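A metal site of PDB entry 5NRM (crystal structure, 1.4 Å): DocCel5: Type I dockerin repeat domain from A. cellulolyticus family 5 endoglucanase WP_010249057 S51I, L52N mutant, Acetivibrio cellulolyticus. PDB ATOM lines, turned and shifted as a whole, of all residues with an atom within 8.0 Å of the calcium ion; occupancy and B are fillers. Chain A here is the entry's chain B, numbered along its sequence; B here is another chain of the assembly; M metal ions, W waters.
The backbone carbonyl oxygen (O) of Ser 10 is bound to the calcium ion.
The calcium ion is bound by OD1 of Asp 4.
The calcium ion is bound by OD1 of Asp 6, 2.4 Å away.
The calcium ion is bound by OD2 of Asp 15, 2.4 Å away.
The side-chain amide oxygen (OD1) of Asn 8 binds the calcium ion, at 2.4 Å.
The calcium ion is bound by water W1 (2.4 Å).
OD1 of Asp 15 binds the calcium ion, 2.5 Å away.
The calcium ion has seven donor atoms within binding distance.
Water W1 lies within hydrogen-bond range of the side-chain amide oxygen (OD1) of Asn 12 (2.7 Å), the side-chain carboxylate (OD2) of Asp 6 (2.7 Å) and the side-chain amide nitrogen (ND2) of Asn 8 (3.2 Å).
The backbone NH (N) of Gly 7 sits close to the side-chain carboxylate (OD1) of Asp 4, at 3.2 Å.
The backbone NH (N) of Gly 9 lies within hydrogen-bond range of the side-chain carboxylate (OD2) of Asp 4 (2.8 Å).
N of Asp 15 is in hydrogen-bond range of OD1 of Asn 12, 3.4 Å away.
The backbone NH of Val 5 sits close to the side-chain carboxylate of Asp 15.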
ATOM      1  N   LYS A   1     -14.649  16.216 -26.042  1.00  0.00           N
ATOM      2  CA  LYS A   1     -14.216  17.196 -27.048  1.00  0.00           C
ATOM      3  C   LYS A   1     -15.342  17.857 -27.864  1.00  0.00           C
ATOM      4  O   LYS A   1     -15.517  19.044 -27.657  1.00  0.00           O
ATOM      5  CB  LYS A   1     -13.019  16.764 -27.906  1.00  0.00           C
ATOM      6  CG  LYS A   1     -12.060  17.933 -27.972  1.00  0.00           C
ATOM      7  CD  LYS A   1     -10.678  17.663 -28.528  1.00  0.00           C
ATOM      8  CE  LYS A   1      -9.917  16.671 -27.634  1.00  0.00           C
ATOM      9  NZ  LYS A   1      -9.898  15.333 -28.263  1.00  0.00           N
ATOM     10  N   GLY A   3     -18.220  20.029 -28.840  1.00  0.00           N
ATOM     11  CA  GLY A   3     -19.018  20.905 -27.978  1.00  0.00           C
ATOM     12  C   GLY A   3     -18.225  21.679 -26.968  1.00  0.00           C
ATOM     13  O   GLY A   3     -18.644  22.736 -26.562  1.00  0.00           O
ATOM     14  N   ASP A   4     -17.039  21.206 -26.652  1.00  0.00           N
ATOM     15  CA  ASP A   4     -16.285  21.844 -25.528  1.00  0.00           C
ATOM     16  C   ASP A   4     -15.358  22.886 -26.184  1.00  0.00           C
ATOM     17  O   ASP A   4     -14.128  22.763 -26.229  1.00  0.00           O
ATOM     18  CB  ASP A   4     -15.478  20.812 -24.767  1.00  0.00           C
ATOM     19  CG  ASP A   4     -14.784  21.422 -23.550  1.00  0.00           C
ATOM     20  OD1 ASP A   4     -15.143  22.530 -23.235  1.00  0.00           O
ATOM     21  OD2 ASP A   4     -13.838  20.781 -23.011  1.00  0.00           O
ATOM     22  N   VAL A   5     -15.945  23.964 -26.705  1.00  0.00           N
ATOM     23  CA  VAL A   5     -15.177  24.986 -27.415  1.00  0.00           C
ATOM     24  C   VAL A   5     -14.189  25.792 -26.572  1.00  0.00           C
ATOM     25  O   VAL A   5     -13.254  26.274 -27.148  1.00  0.00           O
ATOM     26  CB  VAL A   5     -16.125  25.953 -28.252  1.00  0.00           C
ATOM     27  CG1 VAL A   5     -16.983  25.164 -29.210  1.00  0.00           C
ATOM     28  CG2 VAL A   5     -16.953  26.827 -27.384  1.00  0.00           C
ATOM     29  N   ASP A   6     -14.342  25.855 -25.249  1.00  0.00           N
ATOM     30  CA  ASP A   6     -13.313  26.524 -24.435  1.00  0.00           C
ATOM     31  C   ASP A   6     -12.351  25.537 -23.841  1.00  0.00           C
ATOM     32  O   ASP A   6     -11.422  25.966 -23.202  1.00  0.00           O
ATOM     33  CB  ASP A   6     -13.853  27.430 -23.329  1.00  0.00           C
ATOM     34  CG  ASP A   6     -14.634  26.683 -22.238  1.00  0.00           C
ATOM     35  OD1 ASP A   6     -14.620  25.472 -22.176  1.00  0.00           O
ATOM     36  OD2 ASP A   6     -15.235  27.449 -21.441  1.00  0.00           O
ATOM     37  N   GLY A   7     -12.517  24.240 -24.071  1.00  0.00           N
ATOM     38  CA  GLY A   7     -11.510  23.275 -23.657  1.00  0.00           C
ATOM     39  C   GLY A   7     -11.475  22.953 -22.188  1.00  0.00           C
ATOM     40  O   GLY A   7     -10.504  22.278 -21.770  1.00  0.00           O
ATOM     41  N   ASN A   8     -12.474  23.398 -21.427  1.00  0.00           N
ATOM     42  CA  ASN A   8     -12.370  23.269 -19.976  1.00  0.00           C
ATOM     43  C   ASN A   8     -12.756  21.865 -19.457  1.00  0.00           C
ATOM     44  O   ASN A   8     -12.458  21.544 -18.306  1.00  0.00           O
ATOM     45  CB  ASN A   8     -13.094  24.357 -19.204  1.00  0.00           C
ATOM     46  CG  ASN A   8     -14.576  24.202 -19.199  1.00  0.00           C
ATOM     47  OD1 ASN A   8     -15.153  23.422 -19.979  1.00  0.00           O
ATOM     48  ND2 ASN A   8     -15.228  24.916 -18.311  1.00  0.00           N
ATOM     49  N   GLY A   9     -13.226  20.984 -20.329  1.00  0.00           N
ATOM     50  CA  GLY A   9     -13.560  19.607 -19.939  1.00  0.00           C
ATOM     51  C   GLY A   9     -15.076  19.326 -19.896  1.00  0.00           C
ATOM     52  O   GLY A   9     -15.439  18.161 -19.863  1.00  0.00           O
ATOM     53  N   SER A  10     -15.913  20.348 -19.909  1.00  0.00           N
ATOM     54  CA  SER A  10     -17.343  20.144 -19.846  1.00  0.00           C
ATOM     55  C   SER A  10     -18.005  20.979 -20.914  1.00  0.00           C
ATOM     56  O   SER A  10     -17.486  22.056 -21.283  1.00  0.00           O
ATOM     57  CB  SER A  10     -17.848  20.597 -18.487  1.00  0.00           C
ATOM     58  OG  SER A  10     -19.289  20.401 -18.397  1.00  0.00           O
ATOM     59  N   ILE A  11     -19.149  20.503 -21.418  1.00  0.00           N
ATOM     60  CA  ILE A  11     -19.943  21.262 -22.406  1.00  0.00           C
ATOM     61  C   ILE A  11     -21.019  22.000 -21.623  1.00  0.00           C
ATOM     62  O   ILE A  11     -21.873  21.356 -20.958  1.00  0.00           O
ATOM     63  CB  ILE A  11     -20.581  20.284 -23.436  1.00  0.00           C
ATOM     64  CG1 ILE A  11     -19.510  19.493 -24.228  1.00  0.00           C
ATOM     65  CG2 ILE A  11     -21.486  21.110 -24.352  1.00  0.00           C
ATOM     66  CD1 ILE A  11     -20.085  18.279 -24.842  1.00  0.00           C
ATOM     67  N   ASN A  12     -21.033  23.323 -21.678  1.00  0.00           N
ATOM     68  CA  ASN A  12     -21.959  24.074 -20.870  1.00  0.00           C
ATOM     69  C   ASN A  12     -22.333  25.406 -21.543  1.00  0.00           C
ATOM     70  O   ASN A  12     -22.025  25.621 -22.720  1.00  0.00           O
ATOM     71  CB  ASN A  12     -21.407  24.242 -19.426  1.00  0.00           C
ATOM     72  CG  ASN A  12     -20.122  25.088 -19.364  1.00  0.00           C
ATOM     73  OD1 ASN A  12     -19.930  25.997 -20.172  1.00  0.00           O
ATOM     74  ND2 ASN A  12     -19.297  24.816 -18.356  1.00  0.00           N
ATOM     75  N   SER A  13     -23.067  26.231 -20.797  1.00  0.00           N
ATOM     76  CA  SER A  13     -23.609  27.432 -21.392  1.00  0.00           C
ATOM     77  C   SER A  13     -22.549  28.508 -21.722  1.00  0.00           C
ATOM     78  O   SER A  13     -22.801  29.404 -22.532  1.00  0.00           O
ATOM     79  CB  SER A  13     -24.685  28.047 -20.460  1.00  0.00           C
ATOM     80  OG  SER A  13     -24.137  28.386 -19.185  1.00  0.00           O
ATOM     81  N   ILE A  14     -21.373  28.368 -21.143  1.00  0.00           N
ATOM     82  CA  ILE A  14     -20.244  29.243 -21.571  1.00  0.00           C
ATOM     83  C   ILE A  14     -19.714  28.821 -22.966  1.00  0.00           C
ATOM     84  O   ILE A  14     -19.444  29.681 -23.794  1.00  0.00           O
ATOM     85  CB  ILE A  14     -19.150  29.349 -20.497  1.00  0.00           C
ATOM     86  CG1 ILE A  14     -19.749  30.124 -19.263  1.00  0.00           C
ATOM     87  CG2 ILE A  14     -17.903  29.942 -21.087  1.00  0.00           C
ATOM     88  CD1 ILE A  14     -18.849  30.203 -18.029  1.00  0.00           C
ATOM     89  N   ASP A  15     -19.665  27.516 -23.258  1.00  0.00           N
ATOM     90  CA  ASP A  15     -19.369  27.063 -24.641  1.00  0.00           C
ATOM     91  C   ASP A  15     -20.458  27.591 -25.589  1.00  0.00           C
ATOM     92  O   ASP A  15     -20.162  28.097 -26.667  1.00  0.00           O
ATOM     93  CB  ASP A  15     -19.343  25.545 -24.710  1.00  0.00           C
ATOM     94  CG  ASP A  15     -18.267  24.946 -23.817  1.00  0.00           C
ATOM     95  OD1 ASP A  15     -17.081  25.247 -24.026  1.00  0.00           O
ATOM     96  OD2 ASP A  15     -18.627  24.176 -22.878  1.00  0.00           O
ATOM     97  N   PHE A  16     -21.741  27.502 -25.162  1.00  0.00           N
ATOM     98  CA  PHE A  16     -22.828  28.022 -25.997  1.00  0.00           C
ATOM     99  C   PHE A  16     -22.693  29.506 -26.278  1.00  0.00           C
ATOM    100  O   PHE A  16     -22.893  29.942 -27.397  1.00  0.00           O
ATOM    101  CB  PHE A  16     -24.102  27.740 -25.205  1.00  0.00           C
ATOM    102  CG  PHE A  16     -25.435  27.955 -25.898  1.00  0.00           C
ATOM    103  CD1 PHE A  16     -25.715  27.388 -27.101  1.00  0.00           C
ATOM    104  CD2 PHE A  16     -26.427  28.628 -25.248  1.00  0.00           C
ATOM    105  CE1 PHE A  16     -26.975  27.514 -27.651  1.00  0.00           C
ATOM    106  CE2 PHE A  16     -27.704  28.780 -25.820  1.00  0.00           C
ATOM    107  CZ  PHE A  16     -27.952  28.220 -27.038  1.00  0.00           C
ATOM    108  N   LEU A  18     -19.810  31.238 -26.268  1.00  0.00           N
ATOM    109  CA  LEU A  18     -18.699  31.426 -27.146  1.00  0.00           C
ATOM    110  C   LEU A  18     -19.093  31.105 -28.579  1.00  0.00           C
ATOM    111  O   LEU A  18     -18.691  31.803 -29.498  1.00  0.00           O
ATOM    112  CB  LEU A  18     -17.513  30.560 -26.734  1.00  0.00           C
ATOM    113  CG  LEU A  18     -16.848  31.016 -25.412  1.00  0.00           C
ATOM    114  CD1 LEU A  18     -15.938  29.969 -24.870  1.00  0.00           C
ATOM    115  CD2 LEU A  18     -16.026  32.290 -25.549  1.00  0.00           C
ATOM    116  N   MET A  55     -26.221  22.589 -30.175  1.00  0.00           N
ATOM    117  CA  MET A  55     -25.700  22.690 -28.809  1.00  0.00           C
ATOM    118  C   MET A  55     -26.864  22.992 -27.872  1.00  0.00           C
ATOM    119  O   MET A  55     -26.875  22.462 -26.717  1.00  0.00           O
ATOM    120  CB  MET A  55     -24.514  23.663 -28.602  1.00  0.00           C
ATOM    121  CG  MET A  55     -23.796  23.457 -27.126  1.00  0.00           C
ATOM    122  SD  MET A  55     -22.554  24.762 -27.033  1.00  0.00           S
ATOM    123  CE  MET A  55     -21.284  23.640 -27.750  1.00  0.00           C
ATOM    124  N   THR B 120     -23.626  25.936 -14.166  1.00  0.00           N
ATOM    125  CA  THR B 120     -22.759  26.939 -14.713  1.00  0.00           C
ATOM    126  C   THR B 120     -23.454  28.263 -14.974  1.00  0.00           C
ATOM    127  O   THR B 120     -24.551  28.295 -15.514  1.00  0.00           O
ATOM    128  CB  THR B 120     -22.081  26.457 -15.998  1.00  0.00           C
ATOM    129  OG1 THR B 120     -21.316  25.273 -15.704  1.00  0.00           O
ATOM    130  CG2 THR B 120     -21.161  27.552 -16.625  1.00  0.00           C
HETATM  131 CA    CA M   1     -16.436  23.951 -21.938  1.00  0.00          CA
HETATM  132  O   HOH W   1     -17.245  25.775 -20.594  1.00  0.00           O
